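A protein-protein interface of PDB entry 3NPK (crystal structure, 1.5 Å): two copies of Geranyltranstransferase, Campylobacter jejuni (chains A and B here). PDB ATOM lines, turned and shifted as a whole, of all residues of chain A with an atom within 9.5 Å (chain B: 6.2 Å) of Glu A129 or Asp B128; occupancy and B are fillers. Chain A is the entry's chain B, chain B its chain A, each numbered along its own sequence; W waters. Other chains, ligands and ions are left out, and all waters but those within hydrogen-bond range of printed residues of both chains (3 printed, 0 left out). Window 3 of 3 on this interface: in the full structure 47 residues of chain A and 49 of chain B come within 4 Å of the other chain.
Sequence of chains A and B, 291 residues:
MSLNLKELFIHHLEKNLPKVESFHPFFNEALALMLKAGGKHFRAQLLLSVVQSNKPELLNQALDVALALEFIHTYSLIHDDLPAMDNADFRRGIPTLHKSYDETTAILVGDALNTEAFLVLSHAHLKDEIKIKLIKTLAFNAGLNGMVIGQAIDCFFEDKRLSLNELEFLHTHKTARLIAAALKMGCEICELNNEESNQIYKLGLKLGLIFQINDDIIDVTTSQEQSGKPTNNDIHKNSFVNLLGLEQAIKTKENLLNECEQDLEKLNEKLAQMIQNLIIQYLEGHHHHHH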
ATOM      1  N   SER A 122     -23.481   0.165   8.736  1.00  0.00           N
ATOM      2  CA  SER A 122     -23.758  -1.017   7.920  1.00  0.00           C
ATOM      3  C   SER A 122     -24.751  -0.722   6.792  1.00  0.00           C
ATOM      4  O   SER A 122     -24.766  -1.431   5.781  1.00  0.00           O
ATOM      5  CB  SER A 122     -24.225  -2.192   8.783  1.00  0.00           C
ATOM      6  OG  SER A 122     -25.514  -1.958   9.336  1.00  0.00           O
ATOM      7  N   ALA A 124     -24.837   2.251   5.176  1.00  0.00           N
ATOM      8  CA  ALA A 124     -24.302   3.311   4.326  1.00  0.00           C
ATOM      9  C   ALA A 124     -24.357   2.939   2.843  1.00  0.00           C
ATOM     10  O   ALA A 124     -24.303   1.752   2.465  1.00  0.00           O
ATOM     11  CB  ALA A 124     -22.883   3.679   4.747  1.00  0.00           C
ATOM     12  N   LEU A 126     -22.447   2.598   0.395  1.00  0.00           N
ATOM     13  CA  LEU A 126     -21.074   2.315  -0.022  1.00  0.00           C
ATOM     14  C   LEU A 126     -20.945   0.809  -0.206  1.00  0.00           C
ATOM     15  O   LEU A 126     -21.723   0.040   0.356  1.00  0.00           O
ATOM     16  CB  LEU A 126     -20.079   2.792   1.050  1.00  0.00           C
ATOM     17  CG  LEU A 126     -19.980   4.302   1.313  1.00  0.00           C
ATOM     18  CD1 LEU A 126     -19.260   4.586   2.640  1.00  0.00           C
ATOM     19  CD2 LEU A 126     -19.299   5.034   0.137  1.00  0.00           C
ATOM     20  N   LYS A 127     -19.947   0.382  -0.970  1.00  0.00           N
ATOM     21  CA  LYS A 127     -19.697  -1.046  -1.193  1.00  0.00           C
ATOM     22  C   LYS A 127     -19.482  -1.771   0.122  1.00  0.00           C
ATOM     23  O   LYS A 127     -18.879  -1.215   1.042  1.00  0.00           O
ATOM     24  CB  LYS A 127     -18.440  -1.239  -2.039  1.00  0.00           C
ATOM     25  CG  LYS A 127     -18.555  -0.735  -3.448  1.00  0.00           C
ATOM     26  CD  LYS A 127     -17.335  -1.136  -4.249  1.00  0.00           C
ATOM     27  CE  LYS A 127     -16.057  -0.610  -3.625  1.00  0.00           C
ATOM     28  NZ  LYS A 127     -14.934  -0.719  -4.606  1.00  0.00           N
ATOM     29  N   ASP A 128     -19.938  -3.019   0.201  1.00  0.00           N
ATOM     30  CA  ASP A 128     -19.769  -3.799   1.438  1.00  0.00           C
ATOM     31  C   ASP A 128     -18.311  -3.895   1.892  1.00  0.00           C
ATOM     32  O   ASP A 128     -18.031  -3.839   3.091  1.00  0.00           O
ATOM     33  CB  ASP A 128     -20.370  -5.201   1.298  1.00  0.00           C
ATOM     34  CG  ASP A 128     -21.893  -5.188   1.335  1.00  0.00           C
ATOM     35  OD1 ASP A 128     -22.460  -4.170   1.771  1.00  0.00           O
ATOM     36  OD2 ASP A 128     -22.521  -6.184   0.915  1.00  0.00           O
ATOM     37  N   GLU A 129     -17.382  -4.043   0.948  1.00  0.00           N
ATOM     38  CA  GLU A 129     -15.967  -4.142   1.295  1.00  0.00           C
ATOM     39  C   GLU A 129     -15.488  -2.891   2.031  1.00  0.00           C
ATOM     40  O   GLU A 129     -14.724  -2.968   3.012  1.00  0.00           O
ATOM     41  CB  GLU A 129     -15.117  -4.376   0.031  1.00  0.00           C
ATOM     42  CG  GLU A 129     -13.627  -4.433   0.300  1.00  0.00           C
ATOM     43  CD  GLU A 129     -12.792  -4.606  -0.965  1.00  0.00           C
ATOM     44  OE1 GLU A 129     -13.297  -4.329  -2.080  1.00  0.00           O
ATOM     45  OE2 GLU A 129     -11.619  -5.018  -0.837  1.00  0.00           O
ATOM     46  N   ILE A 130     -15.952  -1.734   1.575  1.00  0.00           N
ATOM     47  CA  ILE A 130     -15.608  -0.481   2.226  1.00  0.00           C
ATOM     48  C   ILE A 130     -16.265  -0.393   3.599  1.00  0.00           C
ATOM     49  O   ILE A 130     -15.633   0.010   4.578  1.00  0.00           O
ATOM     50  CB  ILE A 130     -16.045   0.733   1.380  1.00  0.00           C
ATOM     51  CG1 ILE A 130     -15.266   0.779   0.053  1.00  0.00           C
ATOM     52  CG2 ILE A 130     -15.882   2.028   2.180  1.00  0.00           C
ATOM     53  CD1 ILE A 130     -15.694   1.922  -0.809  1.00  0.00           C
ATOM     54  N   LYS A 131     -17.532  -0.792   3.682  1.00  0.00           N
ATOM     55  CA  LYS A 131     -18.241  -0.683   4.959  1.00  0.00           C
ATOM     56  C   LYS A 131     -17.603  -1.574   6.029  1.00  0.00           C
ATOM     57  O   LYS A 131     -17.506  -1.174   7.201  1.00  0.00           O
ATOM     58  CB  LYS A 131     -19.726  -1.002   4.787  1.00  0.00           C
ATOM     59  CG  LYS A 131     -20.438   0.080   3.957  1.00  0.00           C
ATOM     60  CD  LYS A 131     -21.961   0.010   3.983  1.00  0.00           C
ATOM     61  CE  LYS A 131     -22.490  -1.211   3.256  1.00  0.00           C
ATOM     62  NZ  LYS A 131     -23.971  -1.145   3.130  1.00  0.00           N
ATOM     63  N   ILE A 132     -17.155  -2.769   5.640  1.00  0.00           N
ATOM     64  CA  ILE A 132     -16.469  -3.621   6.611  1.00  0.00           C
ATOM     65  C   ILE A 132     -15.173  -2.965   7.115  1.00  0.00           C
ATOM     66  O   ILE A 132     -14.885  -3.008   8.306  1.00  0.00           O
ATOM     67  CB  ILE A 132     -16.206  -5.040   6.060  1.00  0.00           C
ATOM     68  CG1 ILE A 132     -17.522  -5.826   5.967  1.00  0.00           C
ATOM     69  CG2 ILE A 132     -15.160  -5.791   6.923  1.00  0.00           C
ATOM     70  CD1 ILE A 132     -18.197  -6.058   7.343  1.00  0.00           C
ATOM     71  N   LYS A 133     -14.409  -2.336   6.222  1.00  0.00           N
ATOM     72  CA  LYS A 133     -13.200  -1.625   6.644  1.00  0.00           C
ATOM     73  C   LYS A 133     -13.556  -0.515   7.627  1.00  0.00           C
ATOM     74  O   LYS A 133     -12.890  -0.354   8.653  1.00  0.00           O
ATOM     75  CB  LYS A 133     -12.448  -1.053   5.437  1.00  0.00           C
ATOM     76  CG  LYS A 133     -11.733  -2.122   4.647  1.00  0.00           C
ATOM     77  CD  LYS A 133     -10.943  -1.585   3.477  1.00  0.00           C
ATOM     78  CE  LYS A 133     -10.365  -2.772   2.685  1.00  0.00           C
ATOM     79  NZ  LYS A 133      -9.817  -2.428   1.342  1.00  0.00           N
ATOM     80  N   LEU A 134     -14.626   0.223   7.332  1.00  0.00           N
ATOM     81  CA  LEU A 134     -15.036   1.339   8.189  1.00  0.00           C
ATOM     82  C   LEU A 134     -15.449   0.847   9.568  1.00  0.00           C
ATOM     83  O   LEU A 134     -15.132   1.484  10.586  1.00  0.00           O
ATOM     84  CB  LEU A 134     -16.194   2.107   7.566  1.00  0.00           C
ATOM     85  CG  LEU A 134     -15.855   2.840   6.271  1.00  0.00           C
ATOM     86  CD1 LEU A 134     -17.130   3.448   5.676  1.00  0.00           C
ATOM     87  CD2 LEU A 134     -14.790   3.909   6.500  1.00  0.00           C
ATOM     88  N   ILE A 135     -16.174  -0.271   9.598  1.00  0.00           N
ATOM     89  CA  ILE A 135     -16.617  -0.848  10.866  1.00  0.00           C
ATOM     90  C   ILE A 135     -15.432  -1.336  11.705  1.00  0.00           C
ATOM     91  O   ILE A 135     -15.377  -1.097  12.913  1.00  0.00           O
ATOM     92  CB  ILE A 135     -17.658  -1.954  10.637  1.00  0.00           C
ATOM     93  CG1 ILE A 135     -18.937  -1.309  10.090  1.00  0.00           C
ATOM     94  CG2 ILE A 135     -17.913  -2.760  11.921  1.00  0.00           C
ATOM     95  CD1 ILE A 135     -19.902  -2.294   9.453  1.00  0.00           C
ATOM     96  N   LYS A 136     -14.470  -1.988  11.060  1.00  0.00           N
ATOM     97  CA  LYS A 136     -13.251  -2.386  11.754  1.00  0.00           C
ATOM     98  C   LYS A 136     -12.557  -1.177  12.369  1.00  0.00           C
ATOM     99  O   LYS A 136     -12.110  -1.220  13.507  1.00  0.00           O
ATOM    100  CB  LYS A 136     -12.286  -3.087  10.795  1.00  0.00           C
ATOM    101  CG  LYS A 136     -12.734  -4.474  10.367  1.00  0.00           C
ATOM    102  CD  LYS A 136     -11.738  -5.097   9.358  1.00  0.00           C
ATOM    103  CE  LYS A 136     -12.098  -6.533   9.051  1.00  0.00           C
ATOM    104  NZ  LYS A 136     -11.186  -7.165   8.030  1.00  0.00           N
ATOM    105  N   THR A 137     -12.425  -0.114  11.591  1.00  0.00           N
ATOM    106  CA  THR A 137     -11.733   1.075  12.083  1.00  0.00           C
ATOM    107  C   THR A 137     -12.490   1.700  13.249  1.00  0.00           C
ATOM    108  O   THR A 137     -11.888   2.090  14.259  1.00  0.00           O
ATOM    109  CB  THR A 137     -11.514   2.091  10.947  1.00  0.00           C
ATOM    110  OG1 THR A 137     -10.710   1.462   9.944  1.00  0.00           O
ATOM    111  CG2 THR A 137     -10.803   3.355  11.438  1.00  0.00           C
ATOM    112  N   GLU A 188     -10.559   5.569   3.826  1.00  0.00           N
ATOM    113  CA  GLU A 188     -11.147   4.291   3.453  1.00  0.00           C
ATOM    114  C   GLU A 188     -12.350   4.461   2.515  1.00  0.00           C
ATOM    115  O   GLU A 188     -12.517   3.687   1.582  1.00  0.00           O
ATOM    116  CB  GLU A 188     -11.481   3.485   4.718  1.00  0.00           C
ATOM    117  CG  GLU A 188     -10.191   3.015   5.427  1.00  0.00           C
ATOM    118  CD  GLU A 188     -10.399   2.252   6.745  1.00  0.00           C
ATOM    119  OE1 GLU A 188     -11.333   2.575   7.528  1.00  0.00           O
ATOM    120  OE2 GLU A 188      -9.586   1.332   7.004  1.00  0.00           O
ATOM    121  N   ILE A 189     -13.175   5.475   2.761  1.00  0.00           N
ATOM    122  CA  ILE A 189     -14.298   5.767   1.874  1.00  0.00           C
ATOM    123  C   ILE A 189     -13.777   6.034   0.463  1.00  0.00           C
ATOM    124  O   ILE A 189     -14.365   5.576  -0.525  1.00  0.00           O
ATOM    125  CB  ILE A 189     -15.090   6.996   2.363  1.00  0.00           C
ATOM    126  CG1 ILE A 189     -15.814   6.650   3.666  1.00  0.00           C
ATOM    127  CG2 ILE A 189     -16.082   7.471   1.275  1.00  0.00           C
ATOM    128  CD1 ILE A 189     -16.367   7.875   4.368  1.00  0.00           C
ATOM    129  N   GLU A 191     -11.040   4.922  -0.797  1.00  0.00           N
ATOM    130  CA  GLU A 191     -10.188   3.822  -1.234  1.00  0.00           C
ATOM    131  C   GLU A 191      -8.759   4.289  -1.540  1.00  0.00           C
ATOM    132  O   GLU A 191      -8.151   3.882  -2.540  1.00  0.00           O
ATOM    133  CB  GLU A 191     -10.833   3.070  -2.406  1.00  0.00           C
ATOM    134  CG  GLU A 191     -12.054   2.250  -1.977  1.00  0.00           C
ATOM    135  CD  GLU A 191     -12.821   1.652  -3.144  1.00  0.00           C
ATOM    136  OE1 GLU A 191     -13.575   2.397  -3.792  1.00  0.00           O
ATOM    137  OE2 GLU A 191     -12.691   0.431  -3.398  1.00  0.00           O
ATOM    138  N   ASN A 194      -3.110   2.002   1.142  1.00  0.00           N
ATOM    139  CA  ASN A 194      -2.934   1.709   2.557  1.00  0.00           C
ATOM    140  C   ASN A 194      -1.837   2.575   3.165  1.00  0.00           C
ATOM    141  O   ASN A 194      -1.935   3.001   4.317  1.00  0.00           O
ATOM    142  CB  ASN A 194      -2.650   0.218   2.769  1.00  0.00           C
ATOM    143  CG  ASN A 194      -3.879  -0.654   2.532  1.00  0.00           C
ATOM    144  OD1 ASN A 194      -4.999  -0.154   2.360  1.00  0.00           O
ATOM    145  ND2 ASN A 194      -3.674  -1.969   2.522  1.00  0.00           N
ATOM    146  N   SER B 122     -16.969  -8.125  12.465  1.00  0.00           N
ATOM    147  CA  SER B 122     -16.369  -7.581  11.254  1.00  0.00           C
ATOM    148  C   SER B 122     -15.103  -8.334  10.835  1.00  0.00           C
ATOM    149  O   SER B 122     -14.719  -8.289   9.664  1.00  0.00           O
ATOM    150  CB  SER B 122     -16.102  -6.083  11.401  1.00  0.00           C
ATOM    151  OG  SER B 122     -15.037  -5.807  12.297  1.00  0.00           O
ATOM    152  N   LEU B 126     -15.734 -14.732   6.886  1.00  0.00           N
ATOM    153  CA  LEU B 126     -16.917 -14.883   6.045  1.00  0.00           C
ATOM    154  C   LEU B 126     -16.885 -13.752   5.028  1.00  0.00           C
ATOM    155  O   LEU B 126     -16.253 -12.721   5.259  1.00  0.00           O
ATOM    156  CB  LEU B 126     -18.191 -14.749   6.896  1.00  0.00           C
ATOM    157  CG  LEU B 126     -18.396 -15.813   7.967  1.00  0.00           C
ATOM    158  CD1 LEU B 126     -19.499 -15.352   8.965  1.00  0.00           C
ATOM    159  CD2 LEU B 126     -18.780 -17.154   7.319  1.00  0.00           C
ATOM    160  N   LYS B 127     -17.576 -13.928   3.903  1.00  0.00           N
ATOM    161  CA  LYS B 127     -17.637 -12.879   2.897  1.00  0.00           C
ATOM    162  C   LYS B 127     -18.150 -11.577   3.479  1.00  0.00           C
ATOM    163  O   LYS B 127     -19.034 -11.586   4.351  1.00  0.00           O
ATOM    164  CB  LYS B 127     -18.549 -13.296   1.743  1.00  0.00           C
ATOM    165  CG  LYS B 127     -18.018 -14.453   0.926  1.00  0.00           C
ATOM    166  CD  LYS B 127     -18.916 -14.700  -0.256  1.00  0.00           C
ATOM    167  CE  LYS B 127     -20.226 -15.314   0.184  1.00  0.00           C
ATOM    168  NZ  LYS B 127     -20.926 -15.935  -0.982  1.00  0.00           N
ATOM    169  N   ASP B 128     -17.609 -10.464   2.983  1.00  0.00           N
ATOM    170  CA  ASP B 128     -18.029  -9.133   3.444  1.00  0.00           C
ATOM    171  C   ASP B 128     -19.537  -8.923   3.294  1.00  0.00           C
ATOM    172  O   ASP B 128     -20.157  -8.313   4.160  1.00  0.00           O
ATOM    173  CB  ASP B 128     -17.277  -8.007   2.724  1.00  0.00           C
ATOM    174  CG  ASP B 128     -15.830  -7.878   3.187  1.00  0.00           C
ATOM    175  OD1 ASP B 128     -15.508  -8.437   4.263  1.00  0.00           O
ATOM    176  OD2 ASP B 128     -15.017  -7.212   2.493  1.00  0.00           O
ATOM    177  N   GLU B 129     -20.128  -9.430   2.212  1.00  0.00           N
ATOM    178  CA  GLU B 129     -21.565  -9.285   2.015  1.00  0.00           C
ATOM    179  C   GLU B 129     -22.350  -9.943   3.156  1.00  0.00           C
ATOM    180  O   GLU B 129     -23.356  -9.402   3.637  1.00  0.00           O
ATOM    181  CB  GLU B 129     -21.981  -9.885   0.656  1.00  0.00           C
ATOM    182  CG  GLU B 129     -23.471  -9.779   0.343  1.00  0.00           C
ATOM    183  CD  GLU B 129     -23.882 -10.416  -0.994  1.00  0.00           C
ATOM    184  OE1 GLU B 129     -24.981 -10.079  -1.492  1.00  0.00           O
ATOM    185  OE2 GLU B 129     -23.126 -11.252  -1.543  1.00  0.00           O
ATOM    186  N   ILE B 130     -21.901 -11.119   3.579  1.00  0.00           N
ATOM    187  CA  ILE B 130     -22.533 -11.825   4.690  1.00  0.00           C
ATOM    188  C   ILE B 130     -22.322 -11.058   5.993  1.00  0.00           C
ATOM    189  O   ILE B 130     -23.248 -10.886   6.782  1.00  0.00           O
ATOM    190  CB  ILE B 130     -21.956 -13.246   4.841  1.00  0.00           C
ATOM    191  CG1 ILE B 130     -22.332 -14.123   3.637  1.00  0.00           C
ATOM    192  CG2 ILE B 130     -22.406 -13.891   6.161  1.00  0.00           C
ATOM    193  CD1 ILE B 130     -21.672 -15.477   3.685  1.00  0.00           C
ATOM    194  N   LYS B 131     -21.105 -10.573   6.214  1.00  0.00           N
ATOM    195  CA  LYS B 131     -20.816  -9.874   7.462  1.00  0.00           C
ATOM    196  C   LYS B 131     -21.652  -8.599   7.611  1.00  0.00           C
ATOM    197  O   LYS B 131     -22.106  -8.288   8.718  1.00  0.00           O
ATOM    198  CB  LYS B 131     -19.313  -9.605   7.612  1.00  0.00           C
ATOM    199  CG  LYS B 131     -18.524 -10.915   7.739  1.00  0.00           C
ATOM    200  CD  LYS B 131     -17.072 -10.676   8.181  1.00  0.00           C
ATOM    201  CE  LYS B 131     -16.225 -10.013   7.106  1.00  0.00           C
ATOM    202  NZ  LYS B 131     -14.771 -10.010   7.484  1.00  0.00           N
ATOM    203  N   ILE B 132     -21.874  -7.879   6.509  1.00  0.00           N
ATOM    204  CA  ILE B 132     -22.724  -6.686   6.565  1.00  0.00           C
ATOM    205  C   ILE B 132     -24.158  -7.068   6.940  1.00  0.00           C
ATOM    206  O   ILE B 132     -24.775  -6.414   7.782  1.00  0.00           O
ATOM    207  CB  ILE B 132     -22.675  -5.873   5.242  1.00  0.00           C
ATOM    208  CG1 ILE B 132     -21.314  -5.186   5.123  1.00  0.00           C
ATOM    209  CG2 ILE B 132     -23.813  -4.854   5.176  1.00  0.00           C
ATOM    210  CD1 ILE B 132     -21.050  -4.137   6.183  1.00  0.00           C
ATOM    211  N   LYS B 133     -24.674  -8.154   6.356  1.00  0.00           N
ATOM    212  CA  LYS B 133     -26.013  -8.613   6.747  1.00  0.00           C
ATOM    213  C   LYS B 133     -26.067  -8.954   8.229  1.00  0.00           C
ATOM    214  O   LYS B 133     -27.022  -8.585   8.913  1.00  0.00           O
ATOM    215  CB  LYS B 133     -26.455  -9.810   5.914  1.00  0.00           C
ATOM    216  CG  LYS B 133     -26.750  -9.401   4.488  1.00  0.00           C
ATOM    217  CD  LYS B 133     -27.363 -10.517   3.673  1.00  0.00           C
ATOM    218  CE  LYS B 133     -27.629 -10.014   2.252  1.00  0.00           C
ATOM    219  NZ  LYS B 133     -26.378  -9.577   1.579  1.00  0.00           N
HETATM  220  O   HOH W   1     -13.309  -5.249   3.610  1.00  0.00           O
HETATM  221  O   HOH W   2     -24.684  -7.298   2.315  1.00  0.00           O
HETATM  222  O   HOH W   3     -11.720  -9.973   8.168  1.00  0.00           O
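Ser A122 touches Ile B132 (O to CG2, 3.6 Å).
Glu B129 touches Asp A128.
OD1 of Asp A128 touches CG1 of Ile B132, 3.7 Å away.
CA of Glu A129 touches OD2 of Asp B128, 3.4 Å away.
Ile B132 touches Lys A131.
Ser B122 touches Ile A132.
CB of Lys B131 touches CD1 of Ile A132, at 3.7 Å.
CD1 of Ile A132 touches CD1 of Ile B132 (3.6 Å).
Ile A135 touches Ile B132 (CD1 to CD1, 3.9 Å).
Lys A136 touches Ser B122 (CE to O, 3.2 Å).
O of Ser B122 lies within hydrogen-bond range of NZ of Lys B131, 2.8 Å away.
OD1 of Asp B128 lies within salt-bridge range of NZ of Lys B131 (3.7 Å).
The side-chain carboxylate (OE1) of Glu B129 lies within salt-bridge range of the side-chain amino group (NZ) of Lys B133, at 3.4 Å.
O of Ser A122 lies within hydrogen-bond range of NZ of Lys A131, at 2.8 Å.
NZ of Lys A131 lies within salt-bridge range of OD1 of Asp A128 (3.6 Å).
The side-chain carboxylate (OE2) of Glu A129 is in salt-bridge range of the side-chain amino group (NZ) of Lys A133 (3.8 Å).
Water W1 bridges O of Glu A129 (2.8 Å) and OD2 of Asp B128 (2.8 Å).
Water W2 lies within hydrogen-bond range of the side-chain carboxylate of Asp A128 (2.8 Å), the backbone carbonyl oxygen of Glu B129 (2.8 Å) and the side-chain amino group of Lys B133 (2.9 Å).
Water W3 lies within hydrogen-bond range of the side-chain amino group (NZ) of Lys A136 (2.9 Å) and the side-chain amino group (NZ) of Lys B131 (3.1 Å).
Ser A122 touches Ile B132, and with the chains exchanged Ile A132 touches Ser B122.
Asp A128 touches Glu B129, and with the chains exchanged Glu A129 touches Asp B128.
Asp A128 touches Ile B132, and with the chains exchanged Ile A132 touches Asp B128.
Lys A131 touches Ile B132, and with the chains exchanged Ile A132 touches Lys B131.
Positions printed for both chains: 122, 126, 127, 128, 129, 130, 131, 132 and 133.
Of the 12 pairs that touch across the chains among the printed residues, 9 have their exchanged pair printed and touching as well.
Glu A129 touches one residue of chain B.
Asp B128 touches two residues of chain A.
Of the printed residues of chain A, Glu B129 touches Asp A128.
Printed residues of chain B within 4 Å of Ser A122: Ile B132.
The nearest residue of chain B that does not touch Glu A129 is Ile B132 (5.8 Å).
The nearest residue of chain A that does not touch Asp B128 is Asp A128 (4.2 Å).
The nearest printed residue of chain A that does not touch Glu B129 is Ile A132 (5.8 Å).
Of the 9 printed residues of chain B, 5 touch a printed residue of chain A.
Printed residues of chain B that touch a printed residue of chain A: Ser B122, Asp B128, Glu B129, Lys B131 and Ile B132.
Hydrophobic or aromatic side chains of chain B within 4 Å of the printed part of chain A: Ile B132.
Of the 18 printed residues of chain A, 7 touch a printed residue of chain B.
Hydrophobic or aromatic side chains of chain A within 4 Å of the printed part of chain B: Ile A132 and Ile A135.
Among the printed residues, 12 pairs touch across the chains.
Among the printed residues, no Asp or Glu carboxylate lies within 4 Å of a Lys or Arg side-chain nitrogen of the other chain.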
